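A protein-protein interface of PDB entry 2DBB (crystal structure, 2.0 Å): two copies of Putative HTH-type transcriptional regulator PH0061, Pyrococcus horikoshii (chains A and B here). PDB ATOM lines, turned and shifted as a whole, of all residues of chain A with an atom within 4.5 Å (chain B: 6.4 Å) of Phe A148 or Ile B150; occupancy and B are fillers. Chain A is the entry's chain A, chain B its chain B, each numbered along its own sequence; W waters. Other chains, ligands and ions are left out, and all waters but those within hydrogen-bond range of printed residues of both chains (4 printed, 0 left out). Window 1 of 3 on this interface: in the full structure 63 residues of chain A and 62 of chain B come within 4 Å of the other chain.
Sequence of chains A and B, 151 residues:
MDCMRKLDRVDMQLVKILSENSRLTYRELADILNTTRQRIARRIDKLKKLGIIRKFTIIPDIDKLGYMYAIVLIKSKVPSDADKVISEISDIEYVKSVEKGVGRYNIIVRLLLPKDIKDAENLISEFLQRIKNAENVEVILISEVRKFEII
The backbone carbonyl oxygen (O) of Ile A59 sits at hydrogen-bond distance from the backbone NH (N) of Arg B54 (2.8 Å). The backbone NH (N) of Ile A59 is in hydrogen-bond range of the backbone carbonyl oxygen (O) of Lys B55, 2.9 Å away. The side-chain hydroxyl (OH) of Tyr A69 is in hydrogen-bond range of the backbone carbonyl oxygen (O) of Ile B150 (3.1 Å). NZ of Lys A96 is in salt-bridge range of OE1 of Glu B149 (3.6 Å). The side-chain amino group (NZ) of Lys A96 lies within salt-bridge range of the chain-end carboxylate (OXT) of Ile B151, 2.8 Å away. OE1 of Glu B99 is in salt-bridge range of NH2 of Arg A110 (2.7 Å). O of Lys A147 sits at hydrogen-bond distance from N of Val B98 (2.9 Å). NH1 of Arg B54 is in hydrogen-bond range of O of Phe A148 (3.3 Å). The backbone carbonyl oxygen (O) of Lys B96 sits at hydrogen-bond distance from the backbone NH (N) of Glu A149.
The backbone NH (N) of Lys A96 lies within hydrogen-bond range of the backbone carbonyl oxygen (O) of Arg A110 (2.8 Å).
Ile A59 touches Thr B57. O of Pro A60 touches NH2 of Arg B54, at 3.97 Å. CG2 of Ile B150 touches CD of Pro A60, at 3.7 Å. Pro A60 touches Ile B151 (CG to CD1, 3.1 Å). CD1 of Ile B151 touches CD1 of Ile A62, at 3.2 Å. Lys A96 touches Phe B148 (O to C, 3.4 Å). C of Val A145 touches O of Val B98, at 3.8 Å. Val A145 touches Glu B99. O of Lys A147 touches CA of Ser B97, 3.1 Å away. Lys B96 touches Phe A148.
Of the printed residues of chain B, Ile A58 touches Ser B19 (3.97 Å), Lys B55 (3.1 Å) and Ile B150 (3.9 Å). Of the printed residues of chain B, Pro A60 touches Arg B54, Ile B150 and Ile B151. Phe A148 touches three residues of chain B. Ile B150 touches just these residues of chain A: Ile A58 (3.9 Å), Ile A59 (3.8 Å), Pro A60 (3.7 Å), Tyr A69 (3.1 Å), Lys A96 (3.8 Å), Phe A148 (3.6 Å) and Ile A150 (3.4 Å). The nearest residue of chain B that does not touch Phe A148 is Ser B97 (4.1 Å). The nearest printed residue of chain B that does not touch Val A145 is Arg B54 (4.4 Å).
Printed residues of chain B that touch a printed residue of chain A: Ser B19, Arg B54, Lys B55, Thr B57, Ile B59, Lys B96, Ser B97, Val B98, Glu B99, Phe B148, Glu B149, Ile B150 and Ile B151. Hydrophobic or aromatic side chains of chain B within 4 Å of the printed part of chain A: Ile B59, Ile B150 and Ile B151.
Ile A59 touches Ile B150, and with the chains exchanged Ile A150 touches Ile B59. Lys A96 touches Phe B148, and with the chains exchanged Phe A148 touches Lys B96. Lys A96 touches Ile B150, but with the chains exchanged Ile A150 does not touch Lys B96 (4.9 Å). Ile A150 touches its own counterpart, Ile B150. Of the 28 pairs that touch across the chains among the printed residues, 7 have their exchanged pair printed and touching as well.
Water W2 bridges N of Phe A148 (2.6 Å) and NH1 of Arg B54 (3.2 Å). Water W4 lies within hydrogen-bond range of the side-chain hydroxyl (OG) of Ser B97 (2.7 Å) and the guanidinium group (NH2) of Arg A110 (3.1 Å). Water W1 lies within hydrogen-bond range of N of Ile A150, OG1 of Thr B57 and NZ of Lys B55. Water W3 lies within hydrogen-bond range of the guanidinium group of Arg B54, the backbone NH of Ile A62 and the backbone carbonyl oxygen of Pro A60.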
ATOM      1  N   ILE A  58       1.854 -15.928 -24.832  1.00  0.00           N
ATOM      2  CA  ILE A  58       0.454 -16.311 -24.933  1.00  0.00           C
ATOM      3  C   ILE A  58       0.370 -17.742 -25.446  1.00  0.00           C
ATOM      4  O   ILE A  58       1.337 -18.279 -25.991  1.00  0.00           O
ATOM      5  CB  ILE A  58      -0.334 -15.414 -25.928  1.00  0.00           C
ATOM      6  CG1 ILE A  58       0.308 -15.497 -27.317  1.00  0.00           C
ATOM      7  CG2 ILE A  58      -0.397 -13.985 -25.415  1.00  0.00           C
ATOM      8  CD1 ILE A  58      -0.464 -14.777 -28.420  1.00  0.00           C
ATOM      9  N   ILE A  59      -0.791 -18.356 -25.240  1.00  0.00           N
ATOM     10  CA  ILE A  59      -1.055 -19.696 -25.728  1.00  0.00           C
ATOM     11  C   ILE A  59      -2.124 -19.489 -26.800  1.00  0.00           C
ATOM     12  O   ILE A  59      -3.289 -19.236 -26.495  1.00  0.00           O
ATOM     13  CB  ILE A  59      -1.640 -20.636 -24.635  1.00  0.00           C
ATOM     14  CG1 ILE A  59      -0.634 -20.833 -23.496  1.00  0.00           C
ATOM     15  CG2 ILE A  59      -1.993 -21.992 -25.252  1.00  0.00           C
ATOM     16  CD1 ILE A  59       0.720 -21.293 -23.957  1.00  0.00           C
ATOM     17  N   PRO A  60      -1.728 -19.547 -28.073  1.00  0.00           N
ATOM     18  CA  PRO A  60      -2.677 -19.367 -29.175  1.00  0.00           C
ATOM     19  C   PRO A  60      -3.234 -20.707 -29.645  1.00  0.00           C
ATOM     20  O   PRO A  60      -2.705 -21.760 -29.300  1.00  0.00           O
ATOM     21  CB  PRO A  60      -1.821 -18.707 -30.245  1.00  0.00           C
ATOM     22  CG  PRO A  60      -0.522 -19.418 -30.065  1.00  0.00           C
ATOM     23  CD  PRO A  60      -0.339 -19.449 -28.559  1.00  0.00           C
ATOM     24  N   ILE A  62      -3.163 -23.018 -32.245  1.00  0.00           N
ATOM     25  CA  ILE A  62      -2.342 -23.377 -33.396  1.00  0.00           C
ATOM     26  C   ILE A  62      -3.156 -23.718 -34.634  1.00  0.00           C
ATOM     27  O   ILE A  62      -2.850 -23.269 -35.739  1.00  0.00           O
ATOM     28  CB  ILE A  62      -1.422 -24.573 -33.022  1.00  0.00           C
ATOM     29  CG1 ILE A  62      -0.387 -24.100 -32.009  1.00  0.00           C
ATOM     30  CG2 ILE A  62      -0.736 -25.155 -34.248  1.00  0.00           C
ATOM     31  CD1 ILE A  62       0.462 -22.973 -32.524  1.00  0.00           C
ATOM     32  N   TYR A  69       1.289 -29.206 -34.995  1.00  0.00           N
ATOM     33  CA  TYR A  69       2.513 -29.596 -34.325  1.00  0.00           C
ATOM     34  C   TYR A  69       2.959 -30.962 -34.797  1.00  0.00           C
ATOM     35  O   TYR A  69       2.203 -31.712 -35.414  1.00  0.00           O
ATOM     36  CB  TYR A  69       2.326 -29.680 -32.815  1.00  0.00           C
ATOM     37  CG  TYR A  69       2.247 -28.363 -32.089  1.00  0.00           C
ATOM     38  CD1 TYR A  69       3.207 -27.363 -32.291  1.00  0.00           C
ATOM     39  CD2 TYR A  69       1.263 -28.144 -31.129  1.00  0.00           C
ATOM     40  CE1 TYR A  69       3.185 -26.188 -31.541  1.00  0.00           C
ATOM     41  CE2 TYR A  69       1.234 -26.977 -30.380  1.00  0.00           C
ATOM     42  CZ  TYR A  69       2.192 -26.007 -30.584  1.00  0.00           C
ATOM     43  OH  TYR A  69       2.154 -24.866 -29.812  1.00  0.00           O
ATOM     44  N   LYS A  96      10.222 -25.545 -31.872  1.00  0.00           N
ATOM     45  CA  LYS A  96       9.650 -24.830 -30.738  1.00  0.00           C
ATOM     46  C   LYS A  96      10.185 -25.224 -29.375  1.00  0.00           C
ATOM     47  O   LYS A  96      10.187 -24.412 -28.454  1.00  0.00           O
ATOM     48  CB  LYS A  96       8.125 -24.973 -30.739  1.00  0.00           C
ATOM     49  CG  LYS A  96       7.436 -24.558 -32.041  1.00  0.00           C
ATOM     50  CD  LYS A  96       7.502 -23.058 -32.318  1.00  0.00           C
ATOM     51  CE  LYS A  96       8.829 -22.657 -32.925  1.00  0.00           C
ATOM     52  NZ  LYS A  96       8.774 -21.316 -33.564  1.00  0.00           N
ATOM     53  N   ARG A 110       9.688 -30.534 -30.499  1.00  0.00           N
ATOM     54  CA  ARG A 110       8.363 -30.154 -30.970  1.00  0.00           C
ATOM     55  C   ARG A 110       8.560 -29.185 -32.143  1.00  0.00           C
ATOM     56  O   ARG A 110       9.307 -28.210 -32.040  1.00  0.00           O
ATOM     57  CB  ARG A 110       7.550 -29.466 -29.870  1.00  0.00           C
ATOM     58  CG  ARG A 110       6.192 -28.965 -30.376  1.00  0.00           C
ATOM     59  CD  ARG A 110       5.487 -28.092 -29.343  1.00  0.00           C
ATOM     60  NE  ARG A 110       5.058 -28.871 -28.187  1.00  0.00           N
ATOM     61  CZ  ARG A 110       4.057 -29.744 -28.202  1.00  0.00           C
ATOM     62  NH1 ARG A 110       3.368 -29.953 -29.317  1.00  0.00           N
ATOM     63  NH2 ARG A 110       3.746 -30.416 -27.103  1.00  0.00           N
ATOM     64  N   VAL A 145      -4.841 -30.932 -30.263  1.00  0.00           N
ATOM     65  CA  VAL A 145      -4.329 -30.471 -28.978  1.00  0.00           C
ATOM     66  C   VAL A 145      -5.540 -30.388 -28.050  1.00  0.00           C
ATOM     67  O   VAL A 145      -6.405 -29.530 -28.225  1.00  0.00           O
ATOM     68  CB  VAL A 145      -3.691 -29.075 -29.108  1.00  0.00           C
ATOM     69  CG1 VAL A 145      -3.181 -28.598 -27.753  1.00  0.00           C
ATOM     70  CG2 VAL A 145      -2.563 -29.127 -30.129  1.00  0.00           C
ATOM     71  N   LYS A 147      -5.246 -30.154 -24.644  1.00  0.00           N
ATOM     72  CA  LYS A 147      -4.898 -29.322 -23.509  1.00  0.00           C
ATOM     73  C   LYS A 147      -3.483 -28.819 -23.725  1.00  0.00           C
ATOM     74  O   LYS A 147      -2.605 -29.578 -24.149  1.00  0.00           O
ATOM     75  CB  LYS A 147      -4.966 -30.123 -22.203  1.00  0.00           C
ATOM     76  CG  LYS A 147      -4.702 -29.286 -20.970  1.00  0.00           C
ATOM     77  CD  LYS A 147      -4.669 -30.105 -19.695  1.00  0.00           C
ATOM     78  CE  LYS A 147      -4.619 -29.185 -18.477  1.00  0.00           C
ATOM     79  NZ  LYS A 147      -4.631 -29.953 -17.206  1.00  0.00           N
ATOM     80  N   PHE A 148      -3.260 -27.541 -23.449  1.00  0.00           N
ATOM     81  CA  PHE A 148      -1.927 -26.976 -23.611  1.00  0.00           C
ATOM     82  C   PHE A 148      -1.737 -25.820 -22.642  1.00  0.00           C
ATOM     83  O   PHE A 148      -2.337 -24.761 -22.803  1.00  0.00           O
ATOM     84  CB  PHE A 148      -1.718 -26.485 -25.045  1.00  0.00           C
ATOM     85  CG  PHE A 148      -0.270 -26.395 -25.449  1.00  0.00           C
ATOM     86  CD1 PHE A 148       0.357 -27.465 -26.081  1.00  0.00           C
ATOM     87  CD2 PHE A 148       0.472 -25.251 -25.179  1.00  0.00           C
ATOM     88  CE1 PHE A 148       1.709 -27.395 -26.445  1.00  0.00           C
ATOM     89  CE2 PHE A 148       1.823 -25.172 -25.536  1.00  0.00           C
ATOM     90  CZ  PHE A 148       2.439 -26.251 -26.170  1.00  0.00           C
ATOM     91  N   GLU A 149      -0.903 -26.042 -21.632  1.00  0.00           N
ATOM     92  CA  GLU A 149      -0.600 -25.037 -20.622  1.00  0.00           C
ATOM     93  C   GLU A 149       0.887 -25.097 -20.312  1.00  0.00           C
ATOM     94  O   GLU A 149       1.547 -26.090 -20.621  1.00  0.00           O
ATOM     95  CB  GLU A 149      -1.383 -25.319 -19.339  1.00  0.00           C
ATOM     96  CG  GLU A 149      -2.887 -25.290 -19.509  1.00  0.00           C
ATOM     97  CD  GLU A 149      -3.620 -25.627 -18.231  1.00  0.00           C
ATOM     98  OE1 GLU A 149      -4.870 -25.588 -18.238  1.00  0.00           O
ATOM     99  OE2 GLU A 149      -2.949 -25.935 -17.219  1.00  0.00           O
ATOM    100  N   ILE A 150       1.407 -24.036 -19.704  1.00  0.00           N
ATOM    101  CA  ILE A 150       2.815 -23.981 -19.318  1.00  0.00           C
ATOM    102  C   ILE A 150       2.840 -23.788 -17.807  1.00  0.00           C
ATOM    103  O   ILE A 150       3.018 -22.670 -17.319  1.00  0.00           O
ATOM    104  CB  ILE A 150       3.544 -22.782 -19.951  1.00  0.00           C
ATOM    105  CG1 ILE A 150       3.302 -22.748 -21.459  1.00  0.00           C
ATOM    106  CG2 ILE A 150       5.033 -22.880 -19.654  1.00  0.00           C
ATOM    107  CD1 ILE A 150       3.903 -21.548 -22.130  1.00  0.00           C
ATOM    108  N   SER B  19       3.422 -13.071 -28.312  1.00  0.00           N
ATOM    109  CA  SER B  19       4.049 -14.306 -27.883  1.00  0.00           C
ATOM    110  C   SER B  19       5.435 -14.048 -27.291  1.00  0.00           C
ATOM    111  O   SER B  19       5.950 -14.881 -26.542  1.00  0.00           O
ATOM    112  CB  SER B  19       4.133 -15.303 -29.051  1.00  0.00           C
ATOM    113  OG  SER B  19       4.984 -14.842 -30.086  1.00  0.00           O
ATOM    114  N   ARG B  54      -5.823 -18.041 -26.643  1.00  0.00           N
ATOM    115  CA  ARG B  54      -6.523 -18.733 -25.575  1.00  0.00           C
ATOM    116  C   ARG B  54      -6.111 -18.327 -24.173  1.00  0.00           C
ATOM    117  O   ARG B  54      -6.912 -18.408 -23.237  1.00  0.00           O
ATOM    118  CB  ARG B  54      -6.323 -20.239 -25.735  1.00  0.00           C
ATOM    119  CG  ARG B  54      -6.957 -20.826 -26.990  1.00  0.00           C
ATOM    120  CD  ARG B  54      -6.278 -22.131 -27.377  1.00  0.00           C
ATOM    121  NE  ARG B  54      -5.812 -22.856 -26.198  1.00  0.00           N
ATOM    122  CZ  ARG B  54      -5.111 -23.985 -26.230  1.00  0.00           C
ATOM    123  NH1 ARG B  54      -4.732 -24.557 -25.094  1.00  0.00           N
ATOM    124  NH2 ARG B  54      -4.795 -24.545 -27.393  1.00  0.00           N
ATOM    125  N   LYS B  55      -4.872 -17.880 -24.020  1.00  0.00           N
ATOM    126  CA  LYS B  55      -4.388 -17.527 -22.698  1.00  0.00           C
ATOM    127  C   LYS B  55      -3.181 -16.595 -22.737  1.00  0.00           C
ATOM    128  O   LYS B  55      -2.415 -16.585 -23.702  1.00  0.00           O
ATOM    129  CB  LYS B  55      -4.026 -18.828 -21.976  1.00  0.00           C
ATOM    130  CG  LYS B  55      -3.603 -18.710 -20.535  1.00  0.00           C
ATOM    131  CD  LYS B  55      -3.299 -20.101 -19.997  1.00  0.00           C
ATOM    132  CE  LYS B  55      -3.132 -20.104 -18.496  1.00  0.00           C
ATOM    133  NZ  LYS B  55      -2.825 -21.476 -18.000  1.00  0.00           N
ATOM    134  N   THR B  57      -0.028 -16.117 -20.634  1.00  0.00           N
ATOM    135  CA  THR B  57       0.730 -16.794 -19.593  1.00  0.00           C
ATOM    136  C   THR B  57       2.221 -16.445 -19.622  1.00  0.00           C
ATOM    137  O   THR B  57       2.624 -15.457 -20.242  1.00  0.00           O
ATOM    138  CB  THR B  57       0.527 -18.332 -19.720  1.00  0.00           C
ATOM    139  OG1 THR B  57       1.099 -19.001 -18.589  1.00  0.00           O
ATOM    140  CG2 THR B  57       1.167 -18.849 -20.995  1.00  0.00           C
ATOM    141  N   ILE B  59       6.528 -18.112 -19.515  1.00  0.00           N
ATOM    142  CA  ILE B  59       7.419 -19.248 -19.711  1.00  0.00           C
ATOM    143  C   ILE B  59       8.421 -19.153 -18.568  1.00  0.00           C
ATOM    144  O   ILE B  59       9.254 -18.252 -18.525  1.00  0.00           O
ATOM    145  CB  ILE B  59       8.178 -19.180 -21.047  1.00  0.00           C
ATOM    146  CG1 ILE B  59       7.200 -19.333 -22.214  1.00  0.00           C
ATOM    147  CG2 ILE B  59       9.217 -20.291 -21.106  1.00  0.00           C
ATOM    148  CD1 ILE B  59       7.869 -19.292 -23.573  1.00  0.00           C
ATOM    149  N   LYS B  96       0.169 -30.827 -17.945  1.00  0.00           N
ATOM    150  CA  LYS B  96       0.233 -29.563 -18.684  1.00  0.00           C
ATOM    151  C   LYS B  96      -0.252 -29.586 -20.131  1.00  0.00           C
ATOM    152  O   LYS B  96      -0.761 -28.581 -20.640  1.00  0.00           O
ATOM    153  CB  LYS B  96       1.660 -29.005 -18.620  1.00  0.00           C
ATOM    154  CG  LYS B  96       2.151 -28.780 -17.186  1.00  0.00           C
ATOM    155  CD  LYS B  96       1.079 -28.085 -16.360  1.00  0.00           C
ATOM    156  CE  LYS B  96       1.512 -27.870 -14.925  1.00  0.00           C
ATOM    157  NZ  LYS B  96       0.402 -27.258 -14.136  1.00  0.00           N
ATOM    158  N   SER B  97      -0.081 -30.712 -20.810  1.00  0.00           N
ATOM    159  CA  SER B  97      -0.549 -30.804 -22.183  1.00  0.00           C
ATOM    160  C   SER B  97      -0.942 -32.222 -22.531  1.00  0.00           C
ATOM    161  O   SER B  97      -0.413 -33.188 -21.977  1.00  0.00           O
ATOM    162  CB  SER B  97       0.505 -30.297 -23.179  1.00  0.00           C
ATOM    163  OG  SER B  97       1.577 -31.203 -23.339  1.00  0.00           O
ATOM    164  N   VAL B  98      -1.900 -32.324 -23.444  1.00  0.00           N
ATOM    165  CA  VAL B  98      -2.404 -33.600 -23.914  1.00  0.00           C
ATOM    166  C   VAL B  98      -2.664 -33.430 -25.397  1.00  0.00           C
ATOM    167  O   VAL B  98      -3.351 -32.499 -25.825  1.00  0.00           O
ATOM    168  CB  VAL B  98      -3.707 -33.993 -23.187  1.00  0.00           C
ATOM    169  CG1 VAL B  98      -4.225 -35.326 -23.724  1.00  0.00           C
ATOM    170  CG2 VAL B  98      -3.435 -34.105 -21.692  1.00  0.00           C
ATOM    171  N   GLU B  99      -2.092 -34.328 -26.182  1.00  0.00           N
ATOM    172  CA  GLU B  99      -2.230 -34.253 -27.618  1.00  0.00           C
ATOM    173  C   GLU B  99      -2.459 -35.630 -28.220  1.00  0.00           C
ATOM    174  O   GLU B  99      -2.001 -36.640 -27.682  1.00  0.00           O
ATOM    175  CB  GLU B  99      -0.961 -33.615 -28.207  1.00  0.00           C
ATOM    176  CG  GLU B  99      -0.775 -32.136 -27.846  1.00  0.00           C
ATOM    177  CD  GLU B  99       0.639 -31.616 -28.133  1.00  0.00           C
ATOM    178  OE1 GLU B  99       1.587 -32.012 -27.416  1.00  0.00           O
ATOM    179  OE2 GLU B  99       0.812 -30.814 -29.078  1.00  0.00           O
ATOM    180  N   PHE B 148      12.349 -23.731 -25.503  1.00  0.00           N
ATOM    181  CA  PHE B 148      10.935 -23.858 -25.190  1.00  0.00           C
ATOM    182  C   PHE B 148      10.134 -22.621 -25.583  1.00  0.00           C
ATOM    183  O   PHE B 148      10.220 -21.585 -24.929  1.00  0.00           O
ATOM    184  CB  PHE B 148      10.749 -24.128 -23.699  1.00  0.00           C
ATOM    185  CG  PHE B 148       9.458 -24.813 -23.374  1.00  0.00           C
ATOM    186  CD1 PHE B 148       9.393 -26.200 -23.308  1.00  0.00           C
ATOM    187  CD2 PHE B 148       8.299 -24.076 -23.160  1.00  0.00           C
ATOM    188  CE1 PHE B 148       8.189 -26.849 -23.032  1.00  0.00           C
ATOM    189  CE2 PHE B 148       7.087 -24.711 -22.884  1.00  0.00           C
ATOM    190  CZ  PHE B 148       7.031 -26.100 -22.818  1.00  0.00           C
ATOM    191  N   GLU B 149       9.360 -22.741 -26.656  1.00  0.00           N
ATOM    192  CA  GLU B 149       8.515 -21.651 -27.140  1.00  0.00           C
ATOM    193  C   GLU B 149       7.187 -22.263 -27.532  1.00  0.00           C
ATOM    194  O   GLU B 149       7.089 -23.474 -27.707  1.00  0.00           O
ATOM    195  CB  GLU B 149       9.094 -20.987 -28.391  1.00  0.00           C
ATOM    196  CG  GLU B 149      10.530 -20.538 -28.311  1.00  0.00           C
ATOM    197  CD  GLU B 149      10.950 -19.802 -29.574  1.00  0.00           C
ATOM    198  OE1 GLU B 149      10.630 -20.298 -30.681  1.00  0.00           O
ATOM    199  OE2 GLU B 149      11.599 -18.736 -29.460  1.00  0.00           O
ATOM    200  N   ILE B 150       6.169 -21.428 -27.689  1.00  0.00           N
ATOM    201  CA  ILE B 150       4.861 -21.924 -28.094  1.00  0.00           C
ATOM    202  C   ILE B 150       4.732 -21.789 -29.613  1.00  0.00           C
ATOM    203  O   ILE B 150       4.295 -22.720 -30.292  1.00  0.00           O
ATOM    204  CB  ILE B 150       3.727 -21.148 -27.394  1.00  0.00           C
ATOM    205  CG1 ILE B 150       3.957 -21.158 -25.881  1.00  0.00           C
ATOM    206  CG2 ILE B 150       2.382 -21.782 -27.719  1.00  0.00           C
ATOM    207  CD1 ILE B 150       4.250 -22.539 -25.317  1.00  0.00           C
ATOM    208  N   ILE B 151       5.110 -20.625 -30.134  1.00  0.00           N
ATOM    209  CA  ILE B 151       5.080 -20.372 -31.571  1.00  0.00           C
ATOM    210  C   ILE B 151       6.303 -19.549 -31.962  1.00  0.00           C
ATOM    211  O   ILE B 151       6.901 -18.925 -31.058  1.00  0.00           O
ATOM    212  CB  ILE B 151       3.815 -19.595 -31.999  1.00  0.00           C
ATOM    213  CG1 ILE B 151       2.569 -20.428 -31.726  1.00  0.00           C
ATOM    214  CG2 ILE B 151       3.874 -19.276 -33.488  1.00  0.00           C
ATOM    215  CD1 ILE B 151       1.338 -19.905 -32.440  1.00  0.00           C
ATOM    216  OXT ILE B 151       6.645 -19.527 -33.165  1.00  0.00           O
HETATM  217  O   HOH W   1       0.090 -21.769 -18.688  1.00  0.00           O
HETATM  218  O   HOH W   2      -5.228 -26.263 -22.379  1.00  0.00           O
HETATM  219  O   HOH W   3      -2.761 -25.140 -29.810  1.00  0.00           O
HETATM  220  O   HOH W   4       3.699 -29.720 -24.087  1.00  0.00           O
